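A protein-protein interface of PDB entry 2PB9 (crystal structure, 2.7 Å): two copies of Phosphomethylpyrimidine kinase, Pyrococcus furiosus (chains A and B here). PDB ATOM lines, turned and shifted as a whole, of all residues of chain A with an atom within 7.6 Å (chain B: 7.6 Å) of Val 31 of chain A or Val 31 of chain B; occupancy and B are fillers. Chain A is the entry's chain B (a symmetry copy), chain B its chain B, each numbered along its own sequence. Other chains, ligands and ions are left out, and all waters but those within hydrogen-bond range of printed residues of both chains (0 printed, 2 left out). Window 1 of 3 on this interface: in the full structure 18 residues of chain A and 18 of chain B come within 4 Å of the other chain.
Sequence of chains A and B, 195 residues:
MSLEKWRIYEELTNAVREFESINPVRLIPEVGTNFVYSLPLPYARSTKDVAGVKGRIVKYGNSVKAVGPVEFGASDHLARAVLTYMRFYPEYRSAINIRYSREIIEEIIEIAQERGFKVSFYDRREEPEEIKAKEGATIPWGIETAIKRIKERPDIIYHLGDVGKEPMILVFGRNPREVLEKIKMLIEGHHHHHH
Glu 30 of chain A touches Val 31 of chain B, and with the chains exchanged Val 31 of chain A touches Glu 30 of chain B.
Glu 30 of chain A touches Arg 56 of chain B, and with the chains exchanged Arg 56 of chain A touches Glu 30 of chain B.
Gly 164 of chain A touches Glu 166 of chain B, and with the chains exchanged Glu 166 of chain A touches Gly 164 of chain B.
Glu 166 of chain B touches its own counterpart, Glu 166 of chain A.
Positions printed for both chains: 28, 29, 30, 31, 32, 33, 34, 55, 56, 57, 58, 59, 97, 164, 166, 167 and 168.
Of the 12 pairs that touch across the chains among the printed residues, 12 have their exchanged pair printed and touching as well.
Printed residues of chain B that touch a printed residue of chain A: Glu 30, Val 31, Gly 55, Arg 56, Lys 59, Gly 164 and Glu 166.
Hydrophobic or aromatic side chains of chain B within 4 Å of the printed part of chain A: Val 31.
Along chain B the printed residues that touch a printed residue of chain A span positions 30 to 166.
Hydrophobic or aromatic side chains of chain A that line the printed part of chain B: Val 31.
Among the printed residues, Asp or Glu carboxylates within 4 Å of a Lys or Arg side-chain nitrogen of the other chain: Glu 30 of chain A with Arg 56 of chain B (3.1 Å) and Arg 56 of chain A with Glu 30 of chain B (3.1 Å).
NZ of Lys 59 of chain B is in salt-bridge range of OE1 of Glu 30 of chain B (2.4 Å).
The backbone carbonyl oxygen (O) of Val 31 of chain B sits at hydrogen-bond distance from the guanidinium group (NH1) of Arg 56 of chain B (2.6 Å).
The side-chain carboxylate (OE1) of Glu 30 of chain A is in salt-bridge range of the side-chain amino group (NZ) of Lys 59 of chain A.
O of Val 31 of chain A sits at hydrogen-bond distance from NH1 of Arg 56 of chain A.
CA of Val 31 of chain A touches CA of Val 31 of chain B, at 3.9 Å.
Val 31 of chain A touches Glu 166 of chain B.
CA of Gly 55 of chain A touches O of Lys 59 of chain B (3.9 Å).
O of Lys 59 of chain A touches CA of Gly 55 of chain B, at 3.9 Å.
Glu 166 of chain B touches Gly 164 of chain A (CB to O, 3.5 Å).
Glu 166 of chain A touches Val 31 of chain B.
Gly 164 of chain B touches Glu 166 of chain A.
Glu 166 of chain A touches Glu 166 of chain B.
The side-chain carboxylate (OE2) of Glu 30 of chain B lies within salt-bridge range of the guanidinium group (NH2) of Arg 56 of chain A (3.1 Å).
The guanidinium group (NH2) of Arg 56 of chain B lies within salt-bridge range of the side-chain carboxylate (OE2) of Glu 30 of chain A.
O of Glu 30 of chain A sits close to O of Val 31 of chain B (3.3 Å).
The backbone carbonyl oxygen of Glu 30 of chain B sits close to the backbone carbonyl oxygen of Val 31 of chain A, at 3.3 Å.
Val 31 of chain A touches three residues of chain B.
Printed residues of chain B within 4 Å of Arg 56 of chain A: Glu 30 (3.1 Å).
Of the printed residues of chain B, Glu 166 of chain A touches Val 31, Gly 164 and Glu 166.
Met 168 of chain A touches none of the printed residues of chain B.
Of chain A, only Glu 30, Val 31 and Glu 166 come within 4 Å of Val 31 of chain B.
Asn 97 of chain B touches none of the printed residues of chain A.
Of the printed residues of chain A, Glu 166 of chain B touches Val 31 (3.7 Å), Gly 164 (3.5 Å) and Glu 166 (3.97 Å).
The nearest residue of chain A that does not touch Val 31 of chain B is Gly 32 of chain A (5.7 Å).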
ATOM      1  N   ILE A  28     -18.998   7.701   6.968  1.00  0.00           N
ATOM      2  CA  ILE A  28     -17.607   8.106   7.124  1.00  0.00           C
ATOM      3  C   ILE A  28     -17.026   7.498   8.416  1.00  0.00           C
ATOM      4  O   ILE A  28     -17.680   7.517   9.463  1.00  0.00           O
ATOM      5  CB  ILE A  28     -17.481   9.645   7.225  1.00  0.00           C
ATOM      6  CG1 ILE A  28     -18.211  10.321   6.063  1.00  0.00           C
ATOM      7  CG2 ILE A  28     -16.018  10.048   7.229  1.00  0.00           C
ATOM      8  CD1 ILE A  28     -17.600  10.058   4.707  1.00  0.00           C
ATOM      9  N   PRO A  29     -15.802   6.931   8.353  1.00  0.00           N
ATOM     10  CA  PRO A  29     -15.175   6.343   9.542  1.00  0.00           C
ATOM     11  C   PRO A  29     -14.406   7.431  10.316  1.00  0.00           C
ATOM     12  O   PRO A  29     -14.218   8.546   9.813  1.00  0.00           O
ATOM     13  CB  PRO A  29     -14.237   5.297   8.949  1.00  0.00           C
ATOM     14  CG  PRO A  29     -13.745   5.979   7.728  1.00  0.00           C
ATOM     15  CD  PRO A  29     -15.015   6.609   7.146  1.00  0.00           C
ATOM     16  N   GLU A  30     -13.959   7.109  11.527  1.00  0.00           N
ATOM     17  CA  GLU A  30     -13.215   8.067  12.330  1.00  0.00           C
ATOM     18  C   GLU A  30     -11.887   8.445  11.687  1.00  0.00           C
ATOM     19  O   GLU A  30     -11.426   9.582  11.841  1.00  0.00           O
ATOM     20  CB  GLU A  30     -12.975   7.525  13.739  1.00  0.00           C
ATOM     21  CG  GLU A  30     -14.167   7.699  14.666  1.00  0.00           C
ATOM     22  CD  GLU A  30     -14.492   9.171  14.941  1.00  0.00           C
ATOM     23  OE1 GLU A  30     -14.657   9.941  13.966  1.00  0.00           O
ATOM     24  OE2 GLU A  30     -14.590   9.558  16.132  1.00  0.00           O
ATOM     25  N   VAL A  31     -11.280   7.497  10.971  1.00  0.00           N
ATOM     26  CA  VAL A  31     -10.001   7.747  10.296  1.00  0.00           C
ATOM     27  C   VAL A  31     -10.200   8.542   9.020  1.00  0.00           C
ATOM     28  O   VAL A  31      -9.224   8.979   8.413  1.00  0.00           O
ATOM     29  CB  VAL A  31      -9.246   6.439   9.911  1.00  0.00           C
ATOM     30  CG1 VAL A  31      -8.737   5.745  11.158  1.00  0.00           C
ATOM     31  CG2 VAL A  31     -10.160   5.518   9.116  1.00  0.00           C
ATOM     32  N   GLY A  32     -11.462   8.712   8.619  1.00  0.00           N
ATOM     33  CA  GLY A  32     -11.778   9.462   7.417  1.00  0.00           C
ATOM     34  C   GLY A  32     -11.893   8.597   6.176  1.00  0.00           C
ATOM     35  O   GLY A  32     -11.254   7.546   6.061  1.00  0.00           O
ATOM     36  N   THR A  33     -12.712   9.037   5.228  1.00  0.00           N
ATOM     37  CA  THR A  33     -12.888   8.274   4.002  1.00  0.00           C
ATOM     38  C   THR A  33     -11.994   8.780   2.880  1.00  0.00           C
ATOM     39  O   THR A  33     -11.759   9.980   2.755  1.00  0.00           O
ATOM     40  CB  THR A  33     -14.353   8.316   3.518  1.00  0.00           C
ATOM     41  OG1 THR A  33     -15.162   7.505   4.376  1.00  0.00           O
ATOM     42  CG2 THR A  33     -14.460   7.798   2.080  1.00  0.00           C
ATOM     43  N   ASN A  34     -11.472   7.850   2.087  1.00  0.00           N
ATOM     44  CA  ASN A  34     -10.658   8.214   0.942  1.00  0.00           C
ATOM     45  C   ASN A  34     -11.311   7.623  -0.323  1.00  0.00           C
ATOM     46  O   ASN A  34     -11.985   6.591  -0.277  1.00  0.00           O
ATOM     47  CB  ASN A  34      -9.218   7.736   1.106  1.00  0.00           C
ATOM     48  CG  ASN A  34      -8.229   8.638   0.385  1.00  0.00           C
ATOM     49  OD1 ASN A  34      -7.030   8.605   0.659  1.00  0.00           O
ATOM     50  ND2 ASN A  34      -8.726   9.448  -0.535  1.00  0.00           N
ATOM     51  N   GLY A  55      -5.560  14.367   2.594  1.00  0.00           N
ATOM     52  CA  GLY A  55      -6.190  14.623   3.876  1.00  0.00           C
ATOM     53  C   GLY A  55      -7.572  13.993   3.923  1.00  0.00           C
ATOM     54  O   GLY A  55      -8.343  14.220   4.857  1.00  0.00           O
ATOM     55  N   ARG A  56      -7.876  13.203   2.893  1.00  0.00           N
ATOM     56  CA  ARG A  56      -9.155  12.497   2.754  1.00  0.00           C
ATOM     57  C   ARG A  56     -10.381  13.373   2.940  1.00  0.00           C
ATOM     58  O   ARG A  56     -10.307  14.598   2.942  1.00  0.00           O
ATOM     59  CB  ARG A  56      -9.245  11.343   3.755  1.00  0.00           C
ATOM     60  CG  ARG A  56      -8.108  10.375   3.672  1.00  0.00           C
ATOM     61  CD  ARG A  56      -8.004   9.599   4.962  1.00  0.00           C
ATOM     62  NE  ARG A  56      -6.671   9.043   5.114  1.00  0.00           N
ATOM     63  CZ  ARG A  56      -6.130   8.712   6.280  1.00  0.00           C
ATOM     64  NH1 ARG A  56      -6.823   8.883   7.395  1.00  0.00           N
ATOM     65  NH2 ARG A  56      -4.888   8.230   6.327  1.00  0.00           N
ATOM     66  N   ILE A  57     -11.516  12.700   3.084  1.00  0.00           N
ATOM     67  CA  ILE A  57     -12.804  13.334   3.313  1.00  0.00           C
ATOM     68  C   ILE A  57     -13.171  12.900   4.726  1.00  0.00           C
ATOM     69  O   ILE A  57     -13.155  11.703   5.045  1.00  0.00           O
ATOM     70  CB  ILE A  57     -13.855  12.813   2.326  1.00  0.00           C
ATOM     71  CG1 ILE A  57     -13.336  12.984   0.900  1.00  0.00           C
ATOM     72  CG2 ILE A  57     -15.162  13.561   2.515  1.00  0.00           C
ATOM     73  CD1 ILE A  57     -13.911  11.989  -0.101  1.00  0.00           C
ATOM     74  N   VAL A  58     -13.483  13.865   5.580  1.00  0.00           N
ATOM     75  CA  VAL A  58     -13.823  13.550   6.971  1.00  0.00           C
ATOM     76  C   VAL A  58     -15.169  14.113   7.397  1.00  0.00           C
ATOM     77  O   VAL A  58     -15.787  14.897   6.671  1.00  0.00           O
ATOM     78  CB  VAL A  58     -12.747  14.109   7.940  1.00  0.00           C
ATOM     79  CG1 VAL A  58     -11.363  13.633   7.514  1.00  0.00           C
ATOM     80  CG2 VAL A  58     -12.801  15.641   7.961  1.00  0.00           C
ATOM     81  N   LYS A  59     -15.616  13.710   8.582  1.00  0.00           N
ATOM     82  CA  LYS A  59     -16.885  14.202   9.118  1.00  0.00           C
ATOM     83  C   LYS A  59     -16.711  15.641   9.605  1.00  0.00           C
ATOM     84  O   LYS A  59     -15.797  15.925  10.375  1.00  0.00           O
ATOM     85  CB  LYS A  59     -17.345  13.353  10.305  1.00  0.00           C
ATOM     86  CG  LYS A  59     -17.610  11.902  10.002  1.00  0.00           C
ATOM     87  CD  LYS A  59     -18.341  11.244  11.168  1.00  0.00           C
ATOM     88  CE  LYS A  59     -17.450  11.102  12.406  1.00  0.00           C
ATOM     89  NZ  LYS A  59     -16.322  10.154  12.186  1.00  0.00           N
ATOM     90  N   ASN A  97     -13.380   3.654   0.724  1.00  0.00           N
ATOM     91  CA  ASN A  97     -13.458   2.941   1.989  1.00  0.00           C
ATOM     92  C   ASN A  97     -14.465   3.657   2.876  1.00  0.00           C
ATOM     93  O   ASN A  97     -14.358   4.860   3.096  1.00  0.00           O
ATOM     94  CB  ASN A  97     -12.082   2.927   2.656  1.00  0.00           C
ATOM     95  CG  ASN A  97     -11.671   4.296   3.179  1.00  0.00           C
ATOM     96  OD1 ASN A  97     -11.970   4.653   4.324  1.00  0.00           O
ATOM     97  ND2 ASN A  97     -11.001   5.078   2.334  1.00  0.00           N
ATOM     98  N   GLY A 164      -6.345  -2.354  17.851  1.00  0.00           N
ATOM     99  CA  GLY A 164      -5.766  -1.127  17.343  1.00  0.00           C
ATOM    100  C   GLY A 164      -6.242  -0.715  15.966  1.00  0.00           C
ATOM    101  O   GLY A 164      -5.967   0.397  15.533  1.00  0.00           O
ATOM    102  N   GLU A 166      -9.608  -0.433  13.234  1.00  0.00           N
ATOM    103  CA  GLU A 166     -11.055  -0.447  13.082  1.00  0.00           C
ATOM    104  C   GLU A 166     -11.541  -1.274  11.891  1.00  0.00           C
ATOM    105  O   GLU A 166     -10.784  -1.592  10.974  1.00  0.00           O
ATOM    106  CB  GLU A 166     -11.570   0.986  12.927  1.00  0.00           C
ATOM    107  CG  GLU A 166     -10.523   2.054  13.154  1.00  0.00           C
ATOM    108  CD  GLU A 166     -11.134   3.442  13.317  1.00  0.00           C
ATOM    109  OE1 GLU A 166     -11.804   3.939  12.365  1.00  0.00           O
ATOM    110  OE2 GLU A 166     -10.939   4.027  14.413  1.00  0.00           O
ATOM    111  N   PRO A 167     -12.823  -1.652  11.906  1.00  0.00           N
ATOM    112  CA  PRO A 167     -13.351  -2.433  10.787  1.00  0.00           C
ATOM    113  C   PRO A 167     -13.480  -1.485   9.593  1.00  0.00           C
ATOM    114  O   PRO A 167     -13.474  -0.275   9.770  1.00  0.00           O
ATOM    115  CB  PRO A 167     -14.709  -2.898  11.310  1.00  0.00           C
ATOM    116  CG  PRO A 167     -15.122  -1.761  12.196  1.00  0.00           C
ATOM    117  CD  PRO A 167     -13.848  -1.457  12.946  1.00  0.00           C
ATOM    118  N   MET A 168     -13.597  -2.022   8.389  1.00  0.00           N
ATOM    119  CA  MET A 168     -13.734  -1.178   7.219  1.00  0.00           C
ATOM    120  C   MET A 168     -14.449  -1.899   6.100  1.00  0.00           C
ATOM    121  O   MET A 168     -14.361  -3.124   5.972  1.00  0.00           O
ATOM    122  CB  MET A 168     -12.364  -0.720   6.712  1.00  0.00           C
ATOM    123  CG  MET A 168     -11.841   0.574   7.331  1.00  0.00           C
ATOM    124  SD  MET A 168     -12.969   2.094   6.907  1.00  0.00           S
ATOM    125  CE  MET A 168     -13.440   1.542   5.118  1.00  0.00           C
ATOM    126  N   ILE B  28       0.405  12.828  15.021  1.00  0.00           N
ATOM    127  CA  ILE B  28      -1.007  12.822  14.662  1.00  0.00           C
ATOM    128  C   ILE B  28      -1.479  11.376  14.418  1.00  0.00           C
ATOM    129  O   ILE B  28      -0.785  10.596  13.758  1.00  0.00           O
ATOM    130  CB  ILE B  28      -1.257  13.630  13.365  1.00  0.00           C
ATOM    131  CG1 ILE B  28      -0.635  15.024  13.472  1.00  0.00           C
ATOM    132  CG2 ILE B  28      -2.746  13.739  13.099  1.00  0.00           C
ATOM    133  CD1 ILE B  28      -1.279  15.914  14.509  1.00  0.00           C
ATOM    134  N   PRO B  29      -2.653  10.994  14.964  1.00  0.00           N
ATOM    135  CA  PRO B  29      -3.178   9.638  14.766  1.00  0.00           C
ATOM    136  C   PRO B  29      -4.002   9.584  13.465  1.00  0.00           C
ATOM    137  O   PRO B  29      -4.303  10.626  12.868  1.00  0.00           O
ATOM    138  CB  PRO B  29      -4.050   9.427  15.999  1.00  0.00           C
ATOM    139  CG  PRO B  29      -4.649  10.770  16.188  1.00  0.00           C
ATOM    140  CD  PRO B  29      -3.461  11.715  15.968  1.00  0.00           C
ATOM    141  N   GLU B  30      -4.368   8.381  13.031  1.00  0.00           N
ATOM    142  CA  GLU B  30      -5.155   8.231  11.817  1.00  0.00           C
ATOM    143  C   GLU B  30      -6.536   8.859  11.946  1.00  0.00           C
ATOM    144  O   GLU B  30      -7.084   9.360  10.957  1.00  0.00           O
ATOM    145  CB  GLU B  30      -5.288   6.756  11.435  1.00  0.00           C
ATOM    146  CG  GLU B  30      -4.077   6.208  10.699  1.00  0.00           C
ATOM    147  CD  GLU B  30      -3.864   6.873   9.335  1.00  0.00           C
ATOM    148  OE1 GLU B  30      -3.806   8.124   9.280  1.00  0.00           O
ATOM    149  OE2 GLU B  30      -3.748   6.146   8.317  1.00  0.00           O
ATOM    150  N   VAL B  31      -7.092   8.833  13.159  1.00  0.00           N
ATOM    151  CA  VAL B  31      -8.415   9.417  13.408  1.00  0.00           C
ATOM    152  C   VAL B  31      -8.337  10.928  13.510  1.00  0.00           C
ATOM    153  O   VAL B  31      -9.371  11.592  13.555  1.00  0.00           O
ATOM    154  CB  VAL B  31      -9.074   8.901  14.723  1.00  0.00           C
ATOM    155  CG1 VAL B  31      -9.470   7.447  14.571  1.00  0.00           C
ATOM    156  CG2 VAL B  31      -8.120   9.082  15.896  1.00  0.00           C
ATOM    157  N   GLY B  32      -7.111  11.457  13.554  1.00  0.00           N
ATOM    158  CA  GLY B  32      -6.911  12.892  13.643  1.00  0.00           C
ATOM    159  C   GLY B  32      -6.777  13.398  15.067  1.00  0.00           C
ATOM    160  O   GLY B  32      -7.330  12.824  16.010  1.00  0.00           O
ATOM    161  N   THR B  33      -6.039  14.489  15.234  1.00  0.00           N
ATOM    162  CA  THR B  33      -5.852  15.048  16.564  1.00  0.00           C
ATOM    163  C   THR B  33      -6.832  16.175  16.854  1.00  0.00           C
ATOM    164  O   THR B  33      -7.171  16.956  15.968  1.00  0.00           O
ATOM    165  CB  THR B  33      -4.418  15.586  16.753  1.00  0.00           C
ATOM    166  OG1 THR B  33      -3.508  14.487  16.868  1.00  0.00           O
ATOM    167  CG2 THR B  33      -4.329  16.453  18.013  1.00  0.00           C
ATOM    168  N   ASN B  34      -7.308  16.228  18.094  1.00  0.00           N
ATOM    169  CA  ASN B  34      -8.198  17.297  18.509  1.00  0.00           C
ATOM    170  C   ASN B  34      -7.552  18.028  19.702  1.00  0.00           C
ATOM    171  O   ASN B  34      -6.792  17.444  20.480  1.00  0.00           O
ATOM    172  CB  ASN B  34      -9.584  16.766  18.859  1.00  0.00           C
ATOM    173  CG  ASN B  34     -10.674  17.792  18.597  1.00  0.00           C
ATOM    174  OD1 ASN B  34     -11.854  17.452  18.513  1.00  0.00           O
ATOM    175  ND2 ASN B  34     -10.286  19.049  18.463  1.00  0.00           N
ATOM    176  N   GLY B  55     -13.716  19.132  12.785  1.00  0.00           N
ATOM    177  CA  GLY B  55     -13.055  18.298  11.797  1.00  0.00           C
ATOM    178  C   GLY B  55     -11.625  18.009  12.219  1.00  0.00           C
ATOM    179  O   GLY B  55     -10.836  17.451  11.453  1.00  0.00           O
ATOM    180  N   ARG B  56     -11.300  18.404  13.450  1.00  0.00           N
ATOM    181  CA  ARG B  56      -9.974  18.211  14.048  1.00  0.00           C
ATOM    182  C   ARG B  56      -8.818  18.674  13.179  1.00  0.00           C
ATOM    183  O   ARG B  56      -8.994  19.382  12.192  1.00  0.00           O
ATOM    184  CB  ARG B  56      -9.746  16.736  14.386  1.00  0.00           C
ATOM    185  CG  ARG B  56     -10.800  16.142  15.266  1.00  0.00           C
ATOM    186  CD  ARG B  56     -10.784  14.639  15.137  1.00  0.00           C
ATOM    187  NE  ARG B  56     -12.058  14.080  15.553  1.00  0.00           N
ATOM    188  CZ  ARG B  56     -12.520  12.900  15.157  1.00  0.00           C
ATOM    189  NH1 ARG B  56     -11.796  12.158  14.334  1.00  0.00           N
ATOM    190  NH2 ARG B  56     -13.714  12.477  15.572  1.00  0.00           N
ATOM    191  N   ILE B  57      -7.626  18.259  13.589  1.00  0.00           N
ATOM    192  CA  ILE B  57      -6.387  18.553  12.888  1.00  0.00           C
ATOM    193  C   ILE B  57      -5.926  17.189  12.391  1.00  0.00           C
ATOM    194  O   ILE B  57      -5.828  16.231  13.171  1.00  0.00           O
ATOM    195  CB  ILE B  57      -5.339  19.132  13.845  1.00  0.00           C
ATOM    196  CG1 ILE B  57      -5.931  20.341  14.568  1.00  0.00           C
ATOM    197  CG2 ILE B  57      -4.093  19.527  13.074  1.00  0.00           C
ATOM    198  CD1 ILE B  57      -5.318  20.615  15.936  1.00  0.00           C
ATOM    199  N   VAL B  58      -5.659  17.089  11.096  1.00  0.00           N
ATOM    200  CA  VAL B  58      -5.235  15.811  10.517  1.00  0.00           C
ATOM    201  C   VAL B  58      -3.924  15.907   9.755  1.00  0.00           C
ATOM    202  O   VAL B  58      -3.405  17.003   9.523  1.00  0.00           O
ATOM    203  CB  VAL B  58      -6.311  15.265   9.542  1.00  0.00           C
ATOM    204  CG1 VAL B  58      -7.668  15.215  10.235  1.00  0.00           C
ATOM    205  CG2 VAL B  58      -6.385  16.146   8.290  1.00  0.00           C
ATOM    206  N   LYS B  59      -3.395  14.752   9.364  1.00  0.00           N
ATOM    207  CA  LYS B  59      -2.150  14.713   8.597  1.00  0.00           C
ATOM    208  C   LYS B  59      -2.422  15.146   7.157  1.00  0.00           C
ATOM    209  O   LYS B  59      -3.323  14.614   6.512  1.00  0.00           O
ATOM    210  CB  LYS B  59      -1.570  13.297   8.565  1.00  0.00           C
ATOM    211  CG  LYS B  59      -1.198  12.717   9.903  1.00  0.00           C
ATOM    212  CD  LYS B  59      -0.366  11.451   9.717  1.00  0.00           C
ATOM    213  CE  LYS B  59      -1.188  10.295   9.141  1.00  0.00           C
ATOM    214  NZ  LYS B  59      -2.242   9.825  10.084  1.00  0.00           N
ATOM    215  N   ASN B  97      -5.116  15.037  22.203  1.00  0.00           N
ATOM    216  CA  ASN B  97      -4.925  13.606  22.030  1.00  0.00           C
ATOM    217  C   ASN B  97      -3.944  13.392  20.888  1.00  0.00           C
ATOM    218  O   ASN B  97      -4.142  13.908  19.791  1.00  0.00           O
ATOM    219  CB  ASN B  97      -6.265  12.944  21.708  1.00  0.00           C
ATOM    220  CG  ASN B  97      -6.767  13.287  20.312  1.00  0.00           C
ATOM    221  OD1 ASN B  97      -6.450  12.596  19.338  1.00  0.00           O
ATOM    222  ND2 ASN B  97      -7.535  14.370  20.206  1.00  0.00           N
ATOM    223  N   GLY B 164     -10.890  -2.887  17.274  1.00  0.00           N
ATOM    224  CA  GLY B 164     -11.591  -1.809  16.607  1.00  0.00           C
ATOM    225  C   GLY B 164     -11.210  -0.418  17.064  1.00  0.00           C
ATOM    226  O   GLY B 164     -11.595   0.560  16.433  1.00  0.00           O
ATOM    227  N   GLU B 166      -7.998   2.234  18.301  1.00  0.00           N
ATOM    228  CA  GLU B 166      -6.563   2.470  18.340  1.00  0.00           C
ATOM    229  C   GLU B 166      -6.061   2.989  19.688  1.00  0.00           C
ATOM    230  O   GLU B 166      -6.827   3.481  20.517  1.00  0.00           O
ATOM    231  CB  GLU B 166      -6.176   3.475  17.252  1.00  0.00           C
ATOM    232  CG  GLU B 166      -7.299   3.828  16.302  1.00  0.00           C
ATOM    233  CD  GLU B 166      -6.799   4.558  15.059  1.00  0.00           C
ATOM    234  OE1 GLU B 166      -6.213   5.673  15.189  1.00  0.00           O
ATOM    235  OE2 GLU B 166      -6.996   3.999  13.950  1.00  0.00           O
ATOM    236  N   PRO B 167      -4.752   2.863  19.930  1.00  0.00           N
ATOM    237  CA  PRO B 167      -4.208   3.354  21.197  1.00  0.00           C
ATOM    238  C   PRO B 167      -4.210   4.882  21.128  1.00  0.00           C
ATOM    239  O   PRO B 167      -4.310   5.447  20.048  1.00  0.00           O
ATOM    240  CB  PRO B 167      -2.796   2.774  21.206  1.00  0.00           C
ATOM    241  CG  PRO B 167      -2.442   2.757  19.749  1.00  0.00           C
ATOM    242  CD  PRO B 167      -3.704   2.223  19.117  1.00  0.00           C
ATOM    243  N   MET B 168      -4.100   5.551  22.266  1.00  0.00           N
ATOM    244  CA  MET B 168      -4.084   7.001  22.267  1.00  0.00           C
ATOM    245  C   MET B 168      -3.359   7.542  23.477  1.00  0.00           C
ATOM    246  O   MET B 168      -3.350   6.923  24.545  1.00  0.00           O
ATOM    247  CB  MET B 168      -5.508   7.563  22.254  1.00  0.00           C
ATOM    248  CG  MET B 168      -6.110   7.775  20.867  1.00  0.00           C
ATOM    249  SD  MET B 168      -5.132   9.099  19.841  1.00  0.00           S
ATOM    250  CE  MET B 168      -4.693  10.261  21.319  1.00  0.00           C
